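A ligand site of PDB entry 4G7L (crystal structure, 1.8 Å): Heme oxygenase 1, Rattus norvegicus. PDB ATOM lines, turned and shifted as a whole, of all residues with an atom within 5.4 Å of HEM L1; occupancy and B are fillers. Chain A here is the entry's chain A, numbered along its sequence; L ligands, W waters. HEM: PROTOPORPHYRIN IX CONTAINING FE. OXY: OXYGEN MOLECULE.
NE2 of His 25 binds FE of HEM L1, at 2.1 Å.
O1A of HEM L1 lies within salt-bridge range of NZ of Lys 179, at 2.6 Å.
The side-chain hydroxyl (OH) of Tyr 134 is in hydrogen-bond range of an oxygen (O1D) of HEM L1 (2.6 Å).
NH2 of Arg 183 is in salt-bridge range of O2D of HEM L1 (2.8 Å).
An oxygen (O2) of OXY L2 lies within hydrogen-bond range of the backbone NH of Gly 143.
An iron atom (FE) of HEM L1 is bound by an oxygen (O1) of OXY L2 (1.9 Å).
OE1 of Glu 29 sits at hydrogen-bond distance from ND1 of His 25 (2.8 Å).
The side-chain amino group (NZ) of Lys 179 sits at hydrogen-bond distance from the side-chain hydroxyl (OG) of Ser 142, at 2.9 Å.
The side-chain hydroxyl (OG1) of Thr 21 lies within hydrogen-bond range of the side-chain hydroxyl (OH) of Tyr 134, at 3.2 Å.
O of Glu 29 sits close to OE1 of Gln 38 (3.0 Å).
The side-chain amide oxygen of Gln 38 sits close to the backbone carbonyl oxygen of Met 34.
The side-chain amide oxygen (OD1) of Asn 210 is in hydrogen-bond range of the guanidinium group (NH1) of Arg 136, 2.9 Å away.
The side-chain hydroxyl of Ser 142 is in hydrogen-bond range of the backbone carbonyl oxygen of Leu 138 (2.7 Å).
CB of Lys 18 touches O1D of HEM L1, 3.5 Å away.
Ala 28 touches HEM L1.
Glu 29 touches HEM L1 (CB to C3B, 3.7 Å).
Gln 38 touches HEM L1 (OE1 to CBB, 3.0 Å).
Thr 135 touches HEM L1 (O to CMD, 3.6 Å).
Arg 136 touches HEM L1 (NH1 to CBC, 3.7 Å).
Leu 138 touches HEM L1.
Gly 139 touches HEM L1.
Ser 142 touches HEM L1.
Gly 143 touches HEM L1.
CE2 of Phe 207 touches CAC of HEM L1 (3.5 Å).
Asn 210 touches HEM L1.
CE2 of Phe 214 touches CMC of HEM L1, 3.6 Å away.
Water W1 lies within hydrogen-bond range of an oxygen (O2A) of HEM L1 (2.6 Å) and the side-chain amino group (NZ) of Lys 18 (3.3 Å).
Water W3 lies within hydrogen-bond range of O1D of HEM L1 (2.6 Å), O of Ser 14 (2.8 Å) and NE of Arg 183 (3.2 Å).
Water W2 lies within hydrogen-bond range of NH1 of Arg 183 (3.0 Å) and O1A of HEM L1 (3.4 Å).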
ATOM      1  N   SER A  14      -2.299  24.879 -13.741  1.00  0.00           N
ATOM      2  CA  SER A  14      -2.410  23.677 -14.563  1.00  0.00           C
ATOM      3  C   SER A  14      -1.386  22.589 -14.109  1.00  0.00           C
ATOM      4  O   SER A  14      -1.733  21.406 -13.983  1.00  0.00           O
ATOM      5  CB  SER A  14      -2.214  24.041 -16.008  1.00  0.00           C
ATOM      6  OG  SER A  14      -0.882  24.539 -16.168  1.00  0.00           O
ATOM      7  N   LEU A  17      -2.413  21.230 -10.569  1.00  0.00           N
ATOM      8  CA  LEU A  17      -3.511  20.275 -10.693  1.00  0.00           C
ATOM      9  C   LEU A  17      -2.978  18.945 -11.224  1.00  0.00           C
ATOM     10  O   LEU A  17      -3.345  17.902 -10.685  1.00  0.00           O
ATOM     11  CB  LEU A  17      -4.610  20.811 -11.611  1.00  0.00           C
ATOM     12  CG  LEU A  17      -5.598  21.767 -10.936  1.00  0.00           C
ATOM     13  CD1 LEU A  17      -6.447  22.492 -11.982  1.00  0.00           C
ATOM     14  CD2 LEU A  17      -6.518  20.975 -10.015  1.00  0.00           C
ATOM     15  N   LYS A  18      -2.149  18.988 -12.263  1.00  0.00           N
ATOM     16  CA  LYS A  18      -1.552  17.724 -12.751  1.00  0.00           C
ATOM     17  C   LYS A  18      -0.804  16.953 -11.651  1.00  0.00           C
ATOM     18  O   LYS A  18      -1.018  15.775 -11.466  1.00  0.00           O
ATOM     19  CB  LYS A  18      -0.633  17.904 -13.930  1.00  0.00           C
ATOM     20  CG  LYS A  18      -0.301  16.542 -14.617  1.00  0.00           C
ATOM     21  CD  LYS A  18       0.235  16.672 -16.030  1.00  0.00           C
ATOM     22  CE  LYS A  18       0.713  15.321 -16.611  1.00  0.00           C
ATOM     23  NZ  LYS A  18       1.419  15.644 -17.907  1.00  0.00           N
ATOM     24  N   THR A  21      -3.120  15.570  -8.804  1.00  0.00           N
ATOM     25  CA  THR A  21      -4.072  14.489  -9.189  1.00  0.00           C
ATOM     26  C   THR A  21      -3.406  13.281  -9.881  1.00  0.00           C
ATOM     27  O   THR A  21      -4.064  12.301 -10.168  1.00  0.00           O
ATOM     28  CB  THR A  21      -5.277  15.015 -10.042  1.00  0.00           C
ATOM     29  OG1 THR A  21      -4.810  15.494 -11.314  1.00  0.00           O
ATOM     30  CG2 THR A  21      -6.033  16.065  -9.271  1.00  0.00           C
ATOM     31  N   HIS A  25      -5.182   9.721 -10.124  1.00  0.00           N
ATOM     32  CA  HIS A  25      -5.472   9.325 -11.519  1.00  0.00           C
ATOM     33  C   HIS A  25      -5.154   7.883 -11.722  1.00  0.00           C
ATOM     34  O   HIS A  25      -5.924   7.139 -12.357  1.00  0.00           O
ATOM     35  CB  HIS A  25      -4.780  10.246 -12.547  1.00  0.00           C
ATOM     36  CG  HIS A  25      -5.169   9.928 -13.947  1.00  0.00           C
ATOM     37  ND1 HIS A  25      -4.664   8.825 -14.632  1.00  0.00           N
ATOM     38  CD2 HIS A  25      -6.101  10.512 -14.786  1.00  0.00           C
ATOM     39  CE1 HIS A  25      -5.259   8.849 -15.885  1.00  0.00           C
ATOM     40  NE2 HIS A  25      -6.092   9.835 -15.923  1.00  0.00           N
ATOM     41  N   ALA A  28      -7.707   5.760 -10.224  1.00  0.00           N
ATOM     42  CA  ALA A  28      -8.966   5.841 -10.936  1.00  0.00           C
ATOM     43  C   ALA A  28      -8.897   5.013 -12.230  1.00  0.00           C
ATOM     44  O   ALA A  28      -9.831   4.300 -12.532  1.00  0.00           O
ATOM     45  CB  ALA A  28      -9.340   7.281 -11.283  1.00  0.00           C
ATOM     46  N   GLU A  29      -7.815   5.154 -12.957  1.00  0.00           N
ATOM     47  CA  GLU A  29      -7.717   4.438 -14.261  1.00  0.00           C
ATOM     48  C   GLU A  29      -7.591   2.967 -14.036  1.00  0.00           C
ATOM     49  O   GLU A  29      -7.924   2.171 -14.888  1.00  0.00           O
ATOM     50  CB  GLU A  29      -6.609   5.048 -15.126  1.00  0.00           C
ATOM     51  CG  GLU A  29      -5.208   4.904 -14.609  1.00  0.00           C
ATOM     52  CD  GLU A  29      -4.208   5.660 -15.444  1.00  0.00           C
ATOM     53  OE1 GLU A  29      -3.332   6.420 -14.865  1.00  0.00           O
ATOM     54  OE2 GLU A  29      -4.298   5.341 -16.693  1.00  0.00           O
ATOM     55  N   MET A  34     -13.012   0.175 -14.545  1.00  0.00           N
ATOM     56  CA  MET A  34     -12.224   0.723 -15.719  1.00  0.00           C
ATOM     57  C   MET A  34     -11.282  -0.297 -16.257  1.00  0.00           C
ATOM     58  O   MET A  34     -11.085  -0.349 -17.450  1.00  0.00           O
ATOM     59  CB  MET A  34     -11.437   1.952 -15.375  1.00  0.00           C
ATOM     60  CG  MET A  34     -12.295   3.132 -15.084  1.00  0.00           C
ATOM     61  SD  MET A  34     -13.114   3.521 -16.693  1.00  0.00           S
ATOM     62  CE  MET A  34     -14.351   4.706 -16.257  1.00  0.00           C
ATOM     63  N   GLN A  38     -11.357  -1.464 -19.948  1.00  0.00           N
ATOM     64  CA  GLN A  38     -10.180  -1.332 -20.852  1.00  0.00           C
ATOM     65  C   GLN A  38      -9.826  -2.631 -21.498  1.00  0.00           C
ATOM     66  O   GLN A  38      -9.281  -2.600 -22.563  1.00  0.00           O
ATOM     67  CB  GLN A  38      -8.909  -0.815 -20.165  1.00  0.00           C
ATOM     68  CG  GLN A  38      -8.913   0.667 -19.955  1.00  0.00           C
ATOM     69  CD  GLN A  38      -7.976   1.127 -18.866  1.00  0.00           C
ATOM     70  OE1 GLN A  38      -8.268   1.052 -17.656  1.00  0.00           O
ATOM     71  NE2 GLN A  38      -6.842   1.626 -19.272  1.00  0.00           N
ATOM     72  N   TYR A 134     -12.310  20.675 -14.775  1.00  0.00           N
ATOM     73  CA  TYR A 134     -10.989  20.107 -15.116  1.00  0.00           C
ATOM     74  C   TYR A 134     -11.052  18.577 -15.077  1.00  0.00           C
ATOM     75  O   TYR A 134     -10.692  17.894 -16.066  1.00  0.00           O
ATOM     76  CB  TYR A 134      -9.964  20.593 -14.143  1.00  0.00           C
ATOM     77  CG  TYR A 134      -8.696  19.769 -14.045  1.00  0.00           C
ATOM     78  CD1 TYR A 134      -7.703  19.928 -14.985  1.00  0.00           C
ATOM     79  CD2 TYR A 134      -8.463  18.880 -12.982  1.00  0.00           C
ATOM     80  CE1 TYR A 134      -6.529  19.205 -14.961  1.00  0.00           C
ATOM     81  CE2 TYR A 134      -7.280  18.194 -12.922  1.00  0.00           C
ATOM     82  CZ  TYR A 134      -6.303  18.352 -13.888  1.00  0.00           C
ATOM     83  OH  TYR A 134      -5.123  17.612 -13.747  1.00  0.00           O
ATOM     84  N   THR A 135     -11.515  18.049 -13.919  1.00  0.00           N
ATOM     85  CA  THR A 135     -11.480  16.628 -13.664  1.00  0.00           C
ATOM     86  C   THR A 135     -12.282  15.835 -14.697  1.00  0.00           C
ATOM     87  O   THR A 135     -11.824  14.798 -15.196  1.00  0.00           O
ATOM     88  CB  THR A 135     -12.023  16.325 -12.243  1.00  0.00           C
ATOM     89  OG1 THR A 135     -11.063  16.881 -11.305  1.00  0.00           O
ATOM     90  CG2 THR A 135     -12.103  14.753 -11.994  1.00  0.00           C
ATOM     91  N   ARG A 136     -13.473  16.316 -15.029  1.00  0.00           N
ATOM     92  CA  ARG A 136     -14.280  15.604 -16.024  1.00  0.00           C
ATOM     93  C   ARG A 136     -13.849  15.934 -17.488  1.00  0.00           C
ATOM     94  O   ARG A 136     -13.497  14.980 -18.226  1.00  0.00           O
ATOM     95  CB  ARG A 136     -15.752  15.932 -15.837  1.00  0.00           C
ATOM     96  CG  ARG A 136     -16.386  15.138 -14.688  1.00  0.00           C
ATOM     97  CD  ARG A 136     -16.198  13.635 -14.649  1.00  0.00           C
ATOM     98  NE  ARG A 136     -16.341  13.003 -15.922  1.00  0.00           N
ATOM     99  CZ  ARG A 136     -16.080  11.733 -16.228  1.00  0.00           C
ATOM    100  NH1 ARG A 136     -15.776  10.862 -15.352  1.00  0.00           N
ATOM    101  NH2 ARG A 136     -16.132  11.324 -17.478  1.00  0.00           N
ATOM    102  N   LEU A 138     -11.198  17.374 -19.064  1.00  0.00           N
ATOM    103  CA  LEU A 138      -9.900  17.015 -19.597  1.00  0.00           C
ATOM    104  C   LEU A 138      -9.705  15.496 -19.712  1.00  0.00           C
ATOM    105  O   LEU A 138      -9.037  15.011 -20.591  1.00  0.00           O
ATOM    106  CB  LEU A 138      -8.782  17.687 -18.852  1.00  0.00           C
ATOM    107  CG  LEU A 138      -8.669  19.223 -18.931  1.00  0.00           C
ATOM    108  CD1 LEU A 138      -7.172  19.656 -18.722  1.00  0.00           C
ATOM    109  CD2 LEU A 138      -9.284  19.835 -20.151  1.00  0.00           C
ATOM    110  N   GLY A 139     -10.324  14.750 -18.815  1.00  0.00           N
ATOM    111  CA  GLY A 139     -10.299  13.318 -18.935  1.00  0.00           C
ATOM    112  C   GLY A 139     -11.105  12.822 -20.139  1.00  0.00           C
ATOM    113  O   GLY A 139     -10.694  11.820 -20.847  1.00  0.00           O
ATOM    114  N   SER A 142      -9.054  12.806 -23.026  1.00  0.00           N
ATOM    115  CA  SER A 142      -7.860  11.995 -22.905  1.00  0.00           C
ATOM    116  C   SER A 142      -8.247  10.544 -22.889  1.00  0.00           C
ATOM    117  O   SER A 142      -8.492   9.871 -23.935  1.00  0.00           O
ATOM    118  CB  SER A 142      -7.124  12.455 -21.640  1.00  0.00           C
ATOM    119  OG  SER A 142      -6.849  13.880 -21.632  1.00  0.00           O
ATOM    120  N   GLY A 143      -8.319   9.998 -21.686  1.00  0.00           N
ATOM    121  CA  GLY A 143      -8.766   8.581 -21.549  1.00  0.00           C
ATOM    122  C   GLY A 143     -10.146   8.280 -22.097  1.00  0.00           C
ATOM    123  O   GLY A 143     -10.410   7.180 -22.641  1.00  0.00           O
ATOM    124  N   VAL A 146      -9.833   7.002 -25.593  1.00  0.00           N
ATOM    125  CA  VAL A 146      -9.382   5.565 -25.586  1.00  0.00           C
ATOM    126  C   VAL A 146     -10.587   4.683 -25.267  1.00  0.00           C
ATOM    127  O   VAL A 146     -10.828   3.713 -25.988  1.00  0.00           O
ATOM    128  CB  VAL A 146      -8.286   5.294 -24.559  1.00  0.00           C
ATOM    129  CG1 VAL A 146      -7.934   3.785 -24.567  1.00  0.00           C
ATOM    130  CG2 VAL A 146      -7.073   6.198 -24.947  1.00  0.00           C
ATOM    131  N   LEU A 147     -11.371   5.049 -24.252  1.00  0.00           N
ATOM    132  CA  LEU A 147     -12.543   4.302 -23.896  1.00  0.00           C
ATOM    133  C   LEU A 147     -13.541   4.272 -25.074  1.00  0.00           C
ATOM    134  O   LEU A 147     -14.240   3.271 -25.271  1.00  0.00           O
ATOM    135  CB  LEU A 147     -13.229   4.855 -22.664  1.00  0.00           C
ATOM    136  CG  LEU A 147     -12.400   4.783 -21.330  1.00  0.00           C
ATOM    137  CD1 LEU A 147     -13.218   5.469 -20.213  1.00  0.00           C
ATOM    138  CD2 LEU A 147     -12.119   3.321 -21.049  1.00  0.00           C
ATOM    139  N   LYS A 179      -6.771  20.908 -25.122  1.00  0.00           N
ATOM    140  CA  LYS A 179      -6.342  20.771 -23.744  1.00  0.00           C
ATOM    141  C   LYS A 179      -5.206  21.739 -23.384  1.00  0.00           C
ATOM    142  O   LYS A 179      -5.157  22.284 -22.279  1.00  0.00           O
ATOM    143  CB  LYS A 179      -5.945  19.298 -23.432  1.00  0.00           C
ATOM    144  CG  LYS A 179      -7.066  18.324 -23.353  1.00  0.00           C
ATOM    145  CD  LYS A 179      -6.527  16.893 -23.049  1.00  0.00           C
ATOM    146  CE  LYS A 179      -5.873  16.219 -24.215  1.00  0.00           C
ATOM    147  NZ  LYS A 179      -5.278  14.888 -23.808  1.00  0.00           N
ATOM    148  N   ARG A 183      -5.526  24.413 -20.401  1.00  0.00           N
ATOM    149  CA  ARG A 183      -4.536  24.542 -19.315  1.00  0.00           C
ATOM    150  C   ARG A 183      -3.994  25.970 -19.198  1.00  0.00           C
ATOM    151  O   ARG A 183      -3.882  26.560 -18.111  1.00  0.00           O
ATOM    152  CB  ARG A 183      -3.362  23.604 -19.555  1.00  0.00           C
ATOM    153  CG  ARG A 183      -3.709  22.109 -19.412  1.00  0.00           C
ATOM    154  CD  ARG A 183      -2.449  21.235 -19.517  1.00  0.00           C
ATOM    155  NE  ARG A 183      -2.822  19.805 -19.555  1.00  0.00           N
ATOM    156  CZ  ARG A 183      -2.912  19.102 -20.679  1.00  0.00           C
ATOM    157  NH1 ARG A 183      -2.610  19.645 -21.848  1.00  0.00           N
ATOM    158  NH2 ARG A 183      -3.354  17.844 -20.654  1.00  0.00           N
ATOM    159  N   PHE A 207     -11.873  13.398  -8.241  1.00  0.00           N
ATOM    160  CA  PHE A 207     -11.409  12.071  -8.575  1.00  0.00           C
ATOM    161  C   PHE A 207     -12.007  11.004  -7.667  1.00  0.00           C
ATOM    162  O   PHE A 207     -12.434   9.943  -8.140  1.00  0.00           O
ATOM    163  CB  PHE A 207      -9.870  11.980  -8.612  1.00  0.00           C
ATOM    164  CG  PHE A 207      -9.264  12.349  -9.939  1.00  0.00           C
ATOM    165  CD1 PHE A 207      -8.949  13.678 -10.260  1.00  0.00           C
ATOM    166  CD2 PHE A 207      -8.972  11.382 -10.851  1.00  0.00           C
ATOM    167  CE1 PHE A 207      -8.366  14.028 -11.434  1.00  0.00           C
ATOM    168  CE2 PHE A 207      -8.394  11.724 -12.057  1.00  0.00           C
ATOM    169  CZ  PHE A 207      -8.027  13.008 -12.364  1.00  0.00           C
ATOM    170  N   ASN A 210     -15.531  10.102  -8.509  1.00  0.00           N
ATOM    171  CA  ASN A 210     -15.586   9.216  -9.639  1.00  0.00           C
ATOM    172  C   ASN A 210     -15.258   7.766  -9.274  1.00  0.00           C
ATOM    173  O   ASN A 210     -15.941   6.780  -9.699  1.00  0.00           O
ATOM    174  CB  ASN A 210     -14.648   9.738 -10.755  1.00  0.00           C
ATOM    175  CG  ASN A 210     -15.295  10.853 -11.532  1.00  0.00           C
ATOM    176  OD1 ASN A 210     -16.049  10.599 -12.500  1.00  0.00           O
ATOM    177  ND2 ASN A 210     -14.968  12.071 -11.164  1.00  0.00           N
ATOM    178  N   PHE A 214     -17.532   4.429  -9.694  1.00  0.00           N
ATOM    179  CA  PHE A 214     -17.125   3.165 -10.375  1.00  0.00           C
ATOM    180  C   PHE A 214     -17.148   1.987  -9.487  1.00  0.00           C
ATOM    181  O   PHE A 214     -17.546   0.863  -9.896  1.00  0.00           O
ATOM    182  CB  PHE A 214     -15.754   3.254 -10.988  1.00  0.00           C
ATOM    183  CG  PHE A 214     -15.598   4.403 -11.945  1.00  0.00           C
ATOM    184  CD1 PHE A 214     -16.609   4.848 -12.694  1.00  0.00           C
ATOM    185  CD2 PHE A 214     -14.373   5.021 -12.042  1.00  0.00           C
ATOM    186  CE1 PHE A 214     -16.459   5.910 -13.583  1.00  0.00           C
ATOM    187  CE2 PHE A 214     -14.221   6.065 -12.903  1.00  0.00           C
ATOM    188  CZ  PHE A 214     -15.291   6.524 -13.656  1.00  0.00           C
HETATM  189  CHA HEM L   1      -5.277  12.819 -18.453  1.00  0.00           C
HETATM  190  CHB HEM L   1      -5.844   8.113 -19.586  1.00  0.00           C
HETATM  191  CHC HEM L   1      -9.492   7.722 -16.490  1.00  0.00           C
HETATM  192  CHD HEM L   1      -9.126  12.486 -15.700  1.00  0.00           C
HETATM  193  C1A HEM L   1      -5.080  11.510 -19.039  1.00  0.00           C
HETATM  194  C2A HEM L   1      -3.975  11.240 -19.989  1.00  0.00           C
HETATM  195  C3A HEM L   1      -4.145   9.805 -20.377  1.00  0.00           C
HETATM  196  C4A HEM L   1      -5.305   9.409 -19.557  1.00  0.00           C
HETATM  197  CMA HEM L   1      -3.227   9.015 -21.353  1.00  0.00           C
HETATM  198  CAA HEM L   1      -2.967  12.299 -20.425  1.00  0.00           C
HETATM  199  CBA HEM L   1      -3.453  13.355 -21.436  1.00  0.00           C
HETATM  200  CGA HEM L   1      -2.560  14.601 -21.773  1.00  0.00           C
HETATM  201  O1A HEM L   1      -3.056  15.548 -22.559  1.00  0.00           O
HETATM  202  O2A HEM L   1      -1.419  14.693 -21.169  1.00  0.00           O
HETATM  203  C1B HEM L   1      -6.953   7.627 -18.830  1.00  0.00           C
HETATM  204  C2B HEM L   1      -7.357   6.245 -19.036  1.00  0.00           C
HETATM  205  C3B HEM L   1      -8.451   6.137 -18.170  1.00  0.00           C
HETATM  206  C4B HEM L   1      -8.534   7.427 -17.497  1.00  0.00           C
HETATM  207  CMB HEM L   1      -6.836   5.210 -20.016  1.00  0.00           C
HETATM  208  CAB HEM L   1      -9.377   5.076 -17.789  1.00  0.00           C
HETATM  209  CBB HEM L   1      -9.173   3.861 -18.232  1.00  0.00           C
HETATM  210  C1C HEM L   1      -9.662   9.019 -15.893  1.00  0.00           C
HETATM  211  C2C HEM L   1     -10.774   9.201 -14.925  1.00  0.00           C
HETATM  212  C3C HEM L   1     -10.664  10.631 -14.755  1.00  0.00           C
HETATM  213  C4C HEM L   1      -9.579  11.157 -15.569  1.00  0.00           C
HETATM  214  CMC HEM L   1     -11.697   8.225 -14.229  1.00  0.00           C
HETATM  215  CAC HEM L   1     -11.412  11.490 -13.858  1.00  0.00           C
HETATM  216  CBC HEM L   1     -12.582  11.232 -13.556  1.00  0.00           C
HETATM  217  C1D HEM L   1      -7.982  12.998 -16.357  1.00  0.00           C
HETATM  218  C2D HEM L   1      -7.638  14.406 -16.292  1.00  0.00           C
HETATM  219  C3D HEM L   1      -6.515  14.478 -17.127  1.00  0.00           C
HETATM  220  C4D HEM L   1      -6.363  13.151 -17.601  1.00  0.00           C
HETATM  221  CMD HEM L   1      -8.321  15.514 -15.484  1.00  0.00           C
HETATM  222  CAD HEM L   1      -5.661  15.677 -17.457  1.00  0.00           C
HETATM  223  CBD HEM L   1      -4.435  15.734 -16.576  1.00  0.00           C
HETATM  224  CGD HEM L   1      -3.696  17.056 -16.807  1.00  0.00           C
HETATM  225  O1D HEM L   1      -3.581  17.870 -15.883  1.00  0.00           O
HETATM  226  O2D HEM L   1      -3.161  17.173 -17.916  1.00  0.00           O
HETATM  227  NA  HEM L   1      -5.867  10.372 -18.688  1.00  0.00           N
HETATM  228  NB  HEM L   1      -7.616   8.289 -17.887  1.00  0.00           N
HETATM  229  NC  HEM L   1      -8.979  10.175 -16.329  1.00  0.00           N
HETATM  230  ND  HEM L   1      -7.217  12.284 -17.125  1.00  0.00           N
HETATM  231 FE   HEM L   1      -7.425  10.282 -17.490  1.00  0.00          FE
HETATM  232  O1  OXY L   2      -8.690  10.628 -18.908  1.00  0.00           O
HETATM  233  O2  OXY L   2      -9.676   9.992 -18.944  1.00  0.00           O
HETATM  234  O   HOH W   1      -1.710  15.098 -18.654  1.00  0.00           O
HETATM  235  O   HOH W   2      -2.632  18.289 -24.494  1.00  0.00           O
HETATM  236  O   HOH W   3      -2.560  20.211 -16.346  1.00  0.00           O
HETATM  237  O   HOH W   4      -2.974  11.138 -16.628  1.00  0.00           O
